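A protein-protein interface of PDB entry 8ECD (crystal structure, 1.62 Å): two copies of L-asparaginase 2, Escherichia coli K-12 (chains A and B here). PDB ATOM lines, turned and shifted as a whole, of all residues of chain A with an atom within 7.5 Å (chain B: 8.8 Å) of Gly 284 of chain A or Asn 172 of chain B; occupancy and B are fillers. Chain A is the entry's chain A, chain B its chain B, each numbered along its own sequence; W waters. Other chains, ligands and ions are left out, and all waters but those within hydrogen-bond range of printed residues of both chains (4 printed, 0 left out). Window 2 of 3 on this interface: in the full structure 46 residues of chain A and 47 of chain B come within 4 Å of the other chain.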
ATOM      1  N   ASP A 167      18.905 -17.844 -31.557  1.00  0.00           N
ATOM      2  CA  ASP A 167      17.987 -18.972 -31.819  1.00  0.00           C
ATOM      3  C   ASP A 167      18.592 -20.320 -31.331  1.00  0.00           C
ATOM      4  O   ASP A 167      17.878 -21.295 -31.117  1.00  0.00           O
ATOM      5  CB  ASP A 167      17.590 -19.090 -33.241  1.00  0.00           C
ATOM      6  CG  ASP A 167      16.235 -19.897 -33.409  1.00  0.00           C
ATOM      7  OD1 ASP A 167      15.278 -19.700 -32.612  1.00  0.00           O
ATOM      8  OD2 ASP A 167      16.153 -20.725 -34.330  1.00  0.00           O
ATOM      9  N   VAL A 182      16.295 -23.939 -33.749  1.00  0.00           N
ATOM     10  CA  VAL A 182      15.072 -24.704 -34.016  1.00  0.00           C
ATOM     11  C   VAL A 182      13.951 -23.906 -34.653  1.00  0.00           C
ATOM     12  O   VAL A 182      13.024 -24.563 -35.110  1.00  0.00           O
ATOM     13  CB  VAL A 182      14.604 -25.346 -32.679  1.00  0.00           C
ATOM     14  CG1 VAL A 182      15.615 -26.346 -32.138  1.00  0.00           C
ATOM     15  CG2 VAL A 182      14.257 -24.318 -31.586  1.00  0.00           C
ATOM     16  N   ASN A 183      13.969 -22.574 -34.660  1.00  0.00           N
ATOM     17  CA  ASN A 183      12.881 -21.786 -35.262  1.00  0.00           C
ATOM     18  C   ASN A 183      13.307 -21.241 -36.614  1.00  0.00           C
ATOM     19  O   ASN A 183      12.493 -21.293 -37.563  1.00  0.00           O
ATOM     20  CB  ASN A 183      12.490 -20.643 -34.332  1.00  0.00           C
ATOM     21  CG  ASN A 183      11.976 -21.175 -33.015  1.00  0.00           C
ATOM     22  OD1 ASN A 183      10.936 -21.840 -32.980  1.00  0.00           O
ATOM     23  ND2 ASN A 183      12.704 -20.921 -31.948  1.00  0.00           N
ATOM     24  N   GLY A 253       1.885 -24.901 -23.486  1.00  0.00           N
ATOM     25  CA  GLY A 253       1.493 -24.426 -24.808  1.00  0.00           C
ATOM     26  C   GLY A 253       1.988 -23.043 -25.164  1.00  0.00           C
ATOM     27  O   GLY A 253       3.201 -22.703 -25.025  1.00  0.00           O
ATOM     28  N   ASN A 254       1.078 -22.200 -25.648  1.00  0.00           N
ATOM     29  CA  ASN A 254       1.403 -20.822 -26.096  1.00  0.00           C
ATOM     30  C   ASN A 254       1.429 -19.916 -24.847  1.00  0.00           C
ATOM     31  O   ASN A 254       0.628 -18.962 -24.733  1.00  0.00           O
ATOM     32  CB  ASN A 254       0.444 -20.381 -27.182  1.00  0.00           C
ATOM     33  CG  ASN A 254       0.790 -19.063 -27.818  1.00  0.00           C
ATOM     34  OD1 ASN A 254       1.732 -18.376 -27.439  1.00  0.00           O
ATOM     35  ND2 ASN A 254      -0.011 -18.711 -28.815  1.00  0.00           N
ATOM     36  N   SER A 278       6.933 -16.981 -21.308  1.00  0.00           N
ATOM     37  CA  SER A 278       7.610 -17.865 -22.268  1.00  0.00           C
ATOM     38  C   SER A 278       6.922 -19.197 -22.168  1.00  0.00           C
ATOM     39  O   SER A 278       5.757 -19.285 -21.692  1.00  0.00           O
ATOM     40  CB  SER A 278       9.130 -17.939 -22.000  1.00  0.00           C
ATOM     41  OG  SER A 278       9.824 -18.767 -22.966  1.00  0.00           O
ATOM     42  N   SER A 279       7.537 -20.225 -22.761  1.00  0.00           N
ATOM     43  CA  SER A 279       6.894 -21.546 -22.901  1.00  0.00           C
ATOM     44  C   SER A 279       7.922 -22.645 -22.601  1.00  0.00           C
ATOM     45  O   SER A 279       9.077 -22.546 -23.120  1.00  0.00           O
ATOM     46  CB  SER A 279       6.300 -21.786 -24.278  1.00  0.00           C
ATOM     47  OG  SER A 279       5.724 -23.078 -24.299  1.00  0.00           O
ATOM     48  N   VAL A 281       7.473 -25.339 -24.070  1.00  0.00           N
ATOM     49  CA  VAL A 281       7.436 -25.998 -25.391  1.00  0.00           C
ATOM     50  C   VAL A 281       8.653 -25.568 -26.214  1.00  0.00           C
ATOM     51  O   VAL A 281       9.013 -24.400 -26.232  1.00  0.00           O
ATOM     52  CB  VAL A 281       6.122 -25.678 -26.119  1.00  0.00           C
ATOM     53  CG1 VAL A 281       6.068 -26.205 -27.513  1.00  0.00           C
ATOM     54  CG2 VAL A 281       4.903 -26.165 -25.310  1.00  0.00           C
ATOM     55  N   PRO A 282       9.359 -26.529 -26.791  1.00  0.00           N
ATOM     56  CA  PRO A 282      10.752 -26.269 -27.228  1.00  0.00           C
ATOM     57  C   PRO A 282      10.944 -25.493 -28.510  1.00  0.00           C
ATOM     58  O   PRO A 282      12.035 -25.030 -28.792  1.00  0.00           O
ATOM     59  CB  PRO A 282      11.371 -27.657 -27.419  1.00  0.00           C
ATOM     60  CG  PRO A 282      10.133 -28.551 -27.694  1.00  0.00           C
ATOM     61  CD  PRO A 282       9.089 -27.976 -26.767  1.00  0.00           C
ATOM     62  N   THR A 283       9.894 -25.322 -29.296  1.00  0.00           N
ATOM     63  CA  THR A 283       9.919 -24.520 -30.524  1.00  0.00           C
ATOM     64  C   THR A 283       8.657 -23.688 -30.616  1.00  0.00           C
ATOM     65  O   THR A 283       7.594 -24.077 -30.040  1.00  0.00           O
ATOM     66  CB  THR A 283      10.099 -25.407 -31.772  1.00  0.00           C
ATOM     67  OG1 THR A 283       8.865 -26.063 -32.151  1.00  0.00           O
ATOM     68  CG2 THR A 283      11.185 -26.444 -31.618  1.00  0.00           C
ATOM     69  N   GLY A 284       8.758 -22.619 -31.377  1.00  0.00           N
ATOM     70  CA  GLY A 284       7.593 -21.742 -31.587  1.00  0.00           C
ATOM     71  C   GLY A 284       7.547 -20.556 -30.639  1.00  0.00           C
ATOM     72  O   GLY A 284       8.145 -20.557 -29.592  1.00  0.00           O
ATOM     73  N   ALA A 285       6.849 -19.507 -31.074  1.00  0.00           N
ATOM     74  CA  ALA A 285       6.705 -18.274 -30.281  1.00  0.00           C
ATOM     75  C   ALA A 285       5.620 -18.412 -29.242  1.00  0.00           C
ATOM     76  O   ALA A 285       4.554 -19.052 -29.441  1.00  0.00           O
ATOM     77  CB  ALA A 285       6.381 -17.134 -31.225  1.00  0.00           C
ATOM     78  N   THR A 286       5.869 -17.759 -28.123  1.00  0.00           N
ATOM     79  CA  THR A 286       4.840 -17.326 -27.178  1.00  0.00           C
ATOM     80  C   THR A 286       4.323 -15.979 -27.702  1.00  0.00           C
ATOM     81  O   THR A 286       5.081 -14.991 -27.728  1.00  0.00           O
ATOM     82  CB  THR A 286       5.330 -17.256 -25.737  1.00  0.00           C
ATOM     83  OG1 THR A 286       5.725 -18.529 -25.261  1.00  0.00           O
ATOM     84  CG2 THR A 286       4.222 -16.701 -24.855  1.00  0.00           C
ATOM     85  N   THR A 287       3.113 -16.001 -28.242  1.00  0.00           N
ATOM     86  CA  THR A 287       2.540 -14.853 -28.992  1.00  0.00           C
ATOM     87  C   THR A 287       1.731 -13.939 -28.086  1.00  0.00           C
ATOM     88  O   THR A 287       1.229 -14.332 -27.032  1.00  0.00           O
ATOM     89  CB  THR A 287       1.704 -15.344 -30.177  1.00  0.00           C
ATOM     90  OG1 THR A 287       0.508 -15.911 -29.700  1.00  0.00           O
ATOM     91  CG2 THR A 287       2.402 -16.409 -31.001  1.00  0.00           C
ATOM     92  N   SER A 302       7.196 -13.500 -24.807  1.00  0.00           N
ATOM     93  CA  SER A 302       8.641 -13.689 -25.093  1.00  0.00           C
ATOM     94  C   SER A 302       8.901 -13.892 -26.594  1.00  0.00           C
ATOM     95  O   SER A 302      10.084 -13.950 -26.932  1.00  0.00           O
ATOM     96  CB  SER A 302       9.256 -14.832 -24.290  1.00  0.00           C
ATOM     97  OG  SER A 302       8.736 -16.096 -24.729  1.00  0.00           O
ATOM     98  N   GLY A 303       7.885 -14.152 -27.403  1.00  0.00           N
ATOM     99  CA  GLY A 303       8.125 -14.630 -28.791  1.00  0.00           C
ATOM    100  C   GLY A 303       8.928 -15.930 -28.787  1.00  0.00           C
ATOM    101  O   GLY A 303       8.584 -16.811 -27.976  1.00  0.00           O
ATOM    102  N   THR A 304       9.890 -16.106 -29.709  1.00  0.00           N
ATOM    103  CA  THR A 304      10.587 -17.392 -29.830  1.00  0.00           C
ATOM    104  C   THR A 304      11.620 -17.570 -28.722  1.00  0.00           C
ATOM    105  O   THR A 304      12.184 -18.677 -28.642  1.00  0.00           O
ATOM    106  CB  THR A 304      11.245 -17.580 -31.213  1.00  0.00           C
ATOM    107  OG1 THR A 304      12.223 -16.552 -31.378  1.00  0.00           O
ATOM    108  CG2 THR A 304      10.205 -17.504 -32.328  1.00  0.00           C
ATOM    109  N   LEU A 305      11.833 -16.614 -27.824  1.00  0.00           N
ATOM    110  CA  LEU A 305      12.768 -16.826 -26.737  1.00  0.00           C
ATOM    111  C   LEU A 305      12.241 -17.814 -25.721  1.00  0.00           C
ATOM    112  O   LEU A 305      11.130 -17.620 -25.130  1.00  0.00           O
ATOM    113  CB  LEU A 305      13.092 -15.499 -26.074  1.00  0.00           C
ATOM    114  CG  LEU A 305      13.777 -14.420 -26.923  1.00  0.00           C
ATOM    115  CD1 LEU A 305      13.835 -13.115 -26.121  1.00  0.00           C
ATOM    116  CD2 LEU A 305      15.127 -14.824 -27.432  1.00  0.00           C
ATOM    117  N   ASN A 306      13.012 -18.875 -25.499  1.00  0.00           N
ATOM    118  CA  ASN A 306      12.673 -19.893 -24.496  1.00  0.00           C
ATOM    119  C   ASN A 306      12.924 -19.282 -23.122  1.00  0.00           C
ATOM    120  O   ASN A 306      13.398 -18.141 -23.001  1.00  0.00           O
ATOM    121  CB  ASN A 306      13.426 -21.190 -24.814  1.00  0.00           C
ATOM    122  CG  ASN A 306      14.919 -21.124 -24.628  1.00  0.00           C
ATOM    123  OD1 ASN A 306      15.423 -20.393 -23.772  1.00  0.00           O
ATOM    124  ND2 ASN A 306      15.668 -21.931 -25.385  1.00  0.00           N
ATOM    125  N   THR B  97      -4.709 -29.163 -25.513  1.00  0.00           N
ATOM    126  CA  THR B  97      -3.398 -29.605 -25.947  1.00  0.00           C
ATOM    127  C   THR B  97      -2.291 -29.269 -24.940  1.00  0.00           C
ATOM    128  O   THR B  97      -1.285 -29.980 -24.952  1.00  0.00           O
ATOM    129  CB  THR B  97      -3.063 -29.063 -27.335  1.00  0.00           C
ATOM    130  OG1 THR B  97      -2.916 -27.649 -27.229  1.00  0.00           O
ATOM    131  CG2 THR B  97      -4.077 -29.436 -28.400  1.00  0.00           C
ATOM    132  N   ASP B  98      -2.462 -28.262 -24.120  1.00  0.00           N
ATOM    133  CA  ASP B  98      -1.341 -27.759 -23.289  1.00  0.00           C
ATOM    134  C   ASP B  98      -0.746 -28.837 -22.350  1.00  0.00           C
ATOM    135  O   ASP B  98       0.479 -28.931 -22.217  1.00  0.00           O
ATOM    136  CB  ASP B  98      -1.660 -26.530 -22.566  1.00  0.00           C
ATOM    137  CG  ASP B  98      -1.933 -25.361 -23.417  1.00  0.00           C
ATOM    138  OD1 ASP B  98      -1.673 -25.378 -24.617  1.00  0.00           O
ATOM    139  OD2 ASP B  98      -2.346 -24.301 -22.815  1.00  0.00           O
ATOM    140  N   GLU B 101      -0.102 -34.220 -22.812  1.00  0.00           N
ATOM    141  CA  GLU B 101       0.964 -35.162 -22.636  1.00  0.00           C
ATOM    142  C   GLU B 101       1.071 -35.693 -21.214  1.00  0.00           C
ATOM    143  O   GLU B 101       1.628 -36.760 -21.024  1.00  0.00           O
ATOM    144  CB  GLU B 101       2.287 -34.596 -23.099  1.00  0.00           C
ATOM    145  CG  GLU B 101       2.844 -33.548 -22.188  1.00  0.00           C
ATOM    146  CD  GLU B 101       3.903 -32.736 -22.896  1.00  0.00           C
ATOM    147  OE1 GLU B 101       3.552 -31.883 -23.771  1.00  0.00           O
ATOM    148  OE2 GLU B 101       5.118 -32.982 -22.576  1.00  0.00           O
ATOM    149  N   MET B 123      -5.510 -27.703 -32.221  1.00  0.00           N
ATOM    150  CA  MET B 123      -4.666 -26.497 -32.085  1.00  0.00           C
ATOM    151  C   MET B 123      -5.366 -25.257 -32.591  1.00  0.00           C
ATOM    152  O   MET B 123      -4.896 -24.174 -32.249  1.00  0.00           O
ATOM    153  CB  MET B 123      -3.336 -26.714 -32.826  1.00  0.00           C
ATOM    154  CG  MET B 123      -2.450 -27.743 -32.165  1.00  0.00           C
ATOM    155  SD  MET B 123      -1.862 -27.230 -30.539  1.00  0.00           S
ATOM    156  CE  MET B 123      -0.556 -26.097 -31.056  1.00  0.00           C
ATOM    157  N   THR B 169       4.736 -35.658 -26.829  1.00  0.00           N
ATOM    158  CA  THR B 169       4.913 -34.324 -26.236  1.00  0.00           C
ATOM    159  C   THR B 169       4.568 -33.244 -27.235  1.00  0.00           C
ATOM    160  O   THR B 169       4.616 -33.471 -28.459  1.00  0.00           O
ATOM    161  CB  THR B 169       6.326 -34.181 -25.666  1.00  0.00           C
ATOM    162  OG1 THR B 169       6.485 -32.930 -24.957  1.00  0.00           O
ATOM    163  CG2 THR B 169       7.391 -34.245 -26.737  1.00  0.00           C
ATOM    164  N   LYS B 170       4.193 -32.111 -26.714  1.00  0.00           N
ATOM    165  CA  LYS B 170       3.889 -30.915 -27.509  1.00  0.00           C
ATOM    166  C   LYS B 170       5.187 -30.207 -27.888  1.00  0.00           C
ATOM    167  O   LYS B 170       5.861 -29.653 -26.979  1.00  0.00           O
ATOM    168  CB  LYS B 170       2.926 -29.996 -26.745  1.00  0.00           C
ATOM    169  CG  LYS B 170       2.444 -28.818 -27.538  1.00  0.00           C
ATOM    170  CD  LYS B 170       1.269 -28.101 -26.877  1.00  0.00           C
ATOM    171  CE  LYS B 170       0.734 -27.000 -27.696  1.00  0.00           C
ATOM    172  NZ  LYS B 170      -0.494 -26.462 -27.024  1.00  0.00           N
ATOM    173  N   THR B 171       5.549 -30.198 -29.160  1.00  0.00           N
ATOM    174  CA  THR B 171       6.880 -29.691 -29.560  1.00  0.00           C
ATOM    175  C   THR B 171       6.878 -28.242 -30.058  1.00  0.00           C
ATOM    176  O   THR B 171       8.001 -27.609 -30.126  1.00  0.00           O
ATOM    177  CB  THR B 171       7.484 -30.581 -30.636  1.00  0.00           C
ATOM    178  OG1 THR B 171       6.771 -30.466 -31.881  1.00  0.00           O
ATOM    179  CG2 THR B 171       7.650 -31.998 -30.207  1.00  0.00           C
ATOM    180  N   ASN B 172       5.729 -27.709 -30.434  1.00  0.00           N
ATOM    181  CA  ASN B 172       5.581 -26.342 -30.976  1.00  0.00           C
ATOM    182  C   ASN B 172       4.370 -25.628 -30.399  1.00  0.00           C
ATOM    183  O   ASN B 172       3.324 -26.237 -30.116  1.00  0.00           O
ATOM    184  CB  ASN B 172       5.520 -26.398 -32.494  1.00  0.00           C
ATOM    185  CG  ASN B 172       5.500 -25.022 -33.146  1.00  0.00           C
ATOM    186  OD1 ASN B 172       4.422 -24.417 -33.394  1.00  0.00           O
ATOM    187  ND2 ASN B 172       6.698 -24.553 -33.469  1.00  0.00           N
ATOM    188  N   THR B 173       4.510 -24.358 -30.165  1.00  0.00           N
ATOM    189  CA  THR B 173       3.452 -23.573 -29.467  1.00  0.00           C
ATOM    190  C   THR B 173       2.164 -23.462 -30.308  1.00  0.00           C
ATOM    191  O   THR B 173       1.134 -23.239 -29.647  1.00  0.00           O
ATOM    192  CB  THR B 173       3.951 -22.195 -29.060  1.00  0.00           C
ATOM    193  OG1 THR B 173       4.423 -21.573 -30.267  1.00  0.00           O
ATOM    194  CG2 THR B 173       5.066 -22.262 -28.023  1.00  0.00           C
ATOM    195  N   THR B 174       2.207 -23.460 -31.661  1.00  0.00           N
ATOM    196  CA  THR B 174       1.025 -23.182 -32.476  1.00  0.00           C
ATOM    197  C   THR B 174       0.763 -24.195 -33.605  1.00  0.00           C
ATOM    198  O   THR B 174      -0.381 -24.196 -34.086  1.00  0.00           O
ATOM    199  CB  THR B 174       1.142 -21.787 -33.076  1.00  0.00           C
ATOM    200  OG1 THR B 174       2.327 -21.694 -33.855  1.00  0.00           O
ATOM    201  CG2 THR B 174       1.179 -20.709 -32.014  1.00  0.00           C
ATOM    202  N   ASP B 175       1.754 -24.994 -33.995  1.00  0.00           N
ATOM    203  CA  ASP B 175       1.609 -25.900 -35.138  1.00  0.00           C
ATOM    204  C   ASP B 175       0.587 -27.017 -34.973  1.00  0.00           C
ATOM    205  O   ASP B 175       0.574 -27.689 -33.971  1.00  0.00           O
ATOM    206  CB  ASP B 175       2.988 -26.520 -35.413  1.00  0.00           C
ATOM    207  CG  ASP B 175       3.154 -27.068 -36.822  1.00  0.00           C
ATOM    208  OD1 ASP B 175       2.158 -27.466 -37.444  1.00  0.00           O
ATOM    209  OD2 ASP B 175       4.303 -27.128 -37.288  1.00  0.00           O
ATOM    210  N   VAL B 176      -0.278 -27.192 -35.975  1.00  0.00           N
ATOM    211  CA  VAL B 176      -1.216 -28.336 -35.951  1.00  0.00           C
ATOM    212  C   VAL B 176      -0.453 -29.660 -35.819  1.00  0.00           C
ATOM    213  O   VAL B 176      -1.065 -30.637 -35.336  1.00  0.00           O
ATOM    214  CB  VAL B 176      -2.190 -28.399 -37.140  1.00  0.00           C
ATOM    215  CG1 VAL B 176      -3.152 -27.224 -37.088  1.00  0.00           C
ATOM    216  CG2 VAL B 176      -1.481 -28.472 -38.480  1.00  0.00           C
ATOM    217  N   ALA B 177       0.789 -29.707 -36.310  1.00  0.00           N
ATOM    218  CA  ALA B 177       1.633 -30.933 -36.275  1.00  0.00           C
ATOM    219  C   ALA B 177       2.527 -30.996 -35.029  1.00  0.00           C
ATOM    220  O   ALA B 177       3.451 -31.847 -34.944  1.00  0.00           O
ATOM    221  CB  ALA B 177       2.491 -31.002 -37.525  1.00  0.00           C
ATOM    222  N   THR B 178       2.199 -30.239 -33.996  1.00  0.00           N
ATOM    223  CA  THR B 178       2.997 -30.134 -32.757  1.00  0.00           C
ATOM    224  C   THR B 178       3.271 -31.449 -32.032  1.00  0.00           C
ATOM    225  O   THR B 178       4.368 -31.607 -31.493  1.00  0.00           O
ATOM    226  CB  THR B 178       2.311 -29.138 -31.842  1.00  0.00           C
ATOM    227  OG1 THR B 178       3.195 -28.893 -30.733  1.00  0.00           O
ATOM    228  CG2 THR B 178       0.949 -29.582 -31.335  1.00  0.00           C
ATOM    229  N   PHE B 179       2.322 -32.376 -31.996  1.00  0.00           N
ATOM    230  CA  PHE B 179       2.517 -33.587 -31.173  1.00  0.00           C
ATOM    231  C   PHE B 179       3.415 -34.599 -31.855  1.00  0.00           C
ATOM    232  O   PHE B 179       3.103 -35.089 -32.983  1.00  0.00           O
ATOM    233  CB  PHE B 179       1.201 -34.222 -30.744  1.00  0.00           C
ATOM    234  CG  PHE B 179       0.564 -33.477 -29.618  1.00  0.00           C
ATOM    235  CD1 PHE B 179       0.964 -33.625 -28.307  1.00  0.00           C
ATOM    236  CD2 PHE B 179      -0.404 -32.559 -29.921  1.00  0.00           C
ATOM    237  CE1 PHE B 179       0.403 -32.837 -27.313  1.00  0.00           C
ATOM    238  CE2 PHE B 179      -1.008 -31.793 -28.929  1.00  0.00           C
ATOM    239  CZ  PHE B 179      -0.563 -31.900 -27.633  1.00  0.00           C
ATOM    240  N   LYS B 180       4.507 -34.953 -31.184  1.00  0.00           N
ATOM    241  CA  LYS B 180       5.479 -35.918 -31.702  1.00  0.00           C
ATOM    242  C   LYS B 180       5.989 -36.795 -30.546  1.00  0.00           C
ATOM    243  O   LYS B 180       6.050 -36.319 -29.357  1.00  0.00           O
ATOM    244  CB  LYS B 180       6.678 -35.247 -32.347  1.00  0.00           C
ATOM    245  CG  LYS B 180       6.327 -34.402 -33.554  1.00  0.00           C
ATOM    246  CD  LYS B 180       6.002 -35.353 -34.695  1.00  0.00           C
ATOM    247  CE  LYS B 180       6.148 -34.823 -36.101  1.00  0.00           C
ATOM    248  NZ  LYS B 180       5.237 -33.669 -36.312  1.00  0.00           N
ATOM    249  N   VAL B 182       9.125 -37.850 -29.553  1.00  0.00           N
ATOM    250  CA  VAL B 182      10.404 -37.265 -29.962  1.00  0.00           C
ATOM    251  C   VAL B 182      11.586 -38.209 -29.768  1.00  0.00           C
ATOM    252  O   VAL B 182      12.682 -37.903 -30.332  1.00  0.00           O
ATOM    253  CB  VAL B 182      10.642 -35.909 -29.279  1.00  0.00           C
ATOM    254  CG1 VAL B 182       9.610 -34.878 -29.753  1.00  0.00           C
ATOM    255  CG2 VAL B 182      10.668 -35.975 -27.757  1.00  0.00           C
HETATM  256  O   HOH W   1       9.170 -22.953 -34.733  1.00  0.00           O
HETATM  257  O   HOH W   2      -1.667 -23.097 -25.989  1.00  0.00           O
HETATM  258  O   HOH W   3       2.491 -27.577 -23.369  1.00  0.00           O
HETATM  259  O   HOH W   4       4.556 -20.559 -33.200  1.00  0.00           O
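The backbone carbonyl oxygen (O) of Thr 171 of chain B sits at hydrogen-bond distance from the side-chain hydroxyl (OG1) of Thr 283 of chain A.
O of Thr 283 of chain A is in hydrogen-bond range of N of Thr 173 of chain B (3.1 Å).
OG1 of Thr 283 of chain A lies within hydrogen-bond range of ND2 of Asn 172 of chain B.
The side-chain hydroxyl of Thr 173 of chain B sits at hydrogen-bond distance from the backbone carbonyl oxygen of Ala 285 of chain A (2.7 Å).
The backbone carbonyl oxygen (O) of Thr 178 of chain B sits at hydrogen-bond distance from the side-chain hydroxyl (OG1) of Thr 171 of chain B, at 2.7 Å.
OD1 of Asn 172 of chain B sits at hydrogen-bond distance from N of Asp 175 of chain B, 2.8 Å away.
The side-chain carboxylate (OD1) of Asp 98 of chain B lies within salt-bridge range of the side-chain amino group (NZ) of Lys 170 of chain B (2.9 Å).
NZ of Lys 170 of chain B lies within hydrogen-bond range of OG1 of Thr 97 of chain B, at 2.7 Å.
The side-chain hydroxyl (OG) of Ser 279 of chain A lies within hydrogen-bond range of the backbone NH (N) of Val 281 of chain A.
The backbone carbonyl oxygen of Asn 172 of chain B lies within hydrogen-bond range of the side-chain hydroxyl of Thr 178 of chain B, at 2.7 Å.
Gly 253 of chain A touches Asp 98 of chain B (CA to OD1, 3.3 Å).
CA of Gly 253 of chain A touches NZ of Lys 170 of chain B, at 3.6 Å.
Thr 173 of chain B touches Gly 253 of chain A (CG2 to O, 3.6 Å).
Thr 173 of chain B touches Asn 254 of chain A (O to CB, 3.8 Å).
ND2 of Asn 254 of chain A touches CG2 of Thr 174 of chain B (3.95 Å).
Thr 171 of chain B touches Val 281 of chain A (C to CG1, 3.4 Å).
CG1 of Val 281 of chain A touches N of Asn 172 of chain B, 3.3 Å away.
Pro 282 of chain A touches Lys 170 of chain B.
Asn 172 of chain B touches Gly 284 of chain A.
Gly 284 of chain A touches Thr 173 of chain B (C to OG1, 3.3 Å).
Of chain B, only Asn 172 (3.5 Å) and Thr 173 (3.3 Å) come within 4 Å of Gly 284 of chain A.
Asn 172 of chain B touches three residues of chain A.
Of the printed residues of chain B, Pro 282 of chain A touches Lys 170 (3.6 Å) and Thr 171 (3.4 Å).
Of the printed residues of chain B, Gly 253 of chain A touches Asp 98, Lys 170 and Thr 173.
Printed residues of chain B within 4 Å of Ser 279 of chain A: Thr 173 (3.9 Å).
Of the printed residues of chain A, Thr 173 of chain B touches Gly 253, Asn 254, Ser 279, Val 281, Thr 283, Gly 284 and Ala 285.
Printed residues of chain A within 4 Å of Lys 170 of chain B: Gly 253 (3.6 Å), Val 281 (3.5 Å) and Pro 282 (3.6 Å).
Asn 183 of chain A touches none of the printed residues of chain B.
Thr 97 of chain B touches none of the printed residues of chain A.
The nearest printed residue of chain B that does not touch Gly 253 of chain A is Asn 172 of chain B (5.9 Å).
Printed residues of chain B that touch a printed residue of chain A: Asp 98, Lys 170, Thr 171, Asn 172, Thr 173 and Thr 174.
Hydrophobic or aromatic side chains of chain A within 4 Å of the printed part of chain B: Val 281 and Pro 282.
Among the printed residues, 18 pairs touch across the chains.
1 position is printed for both chains.
Of the 18 pairs that touch across the chains among the printed residues, none has its exchanged pair printed and touching as well.
Water W4 lies within hydrogen-bond range of OG1 of Thr 174 of chain B (2.6 Å), OG1 of Thr 173 of chain B (3.1 Å) and N of Ala 285 of chain A (3.3 Å).
Water W2 bridges OD1 of Asp 98 of chain B (2.7 Å) and N of Asn 254 of chain A (2.9 Å).
Water W3 bridges O of Asp 98 of chain B (2.7 Å) and N of Gly 253 of chain A (2.7 Å).
Water W1 lies within hydrogen-bond range of OD1 of Asn 183 of chain A (2.7 Å), ND2 of Asn 172 of chain B (3.2 Å) and N of Gly 284 of chain A (3.4 Å).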
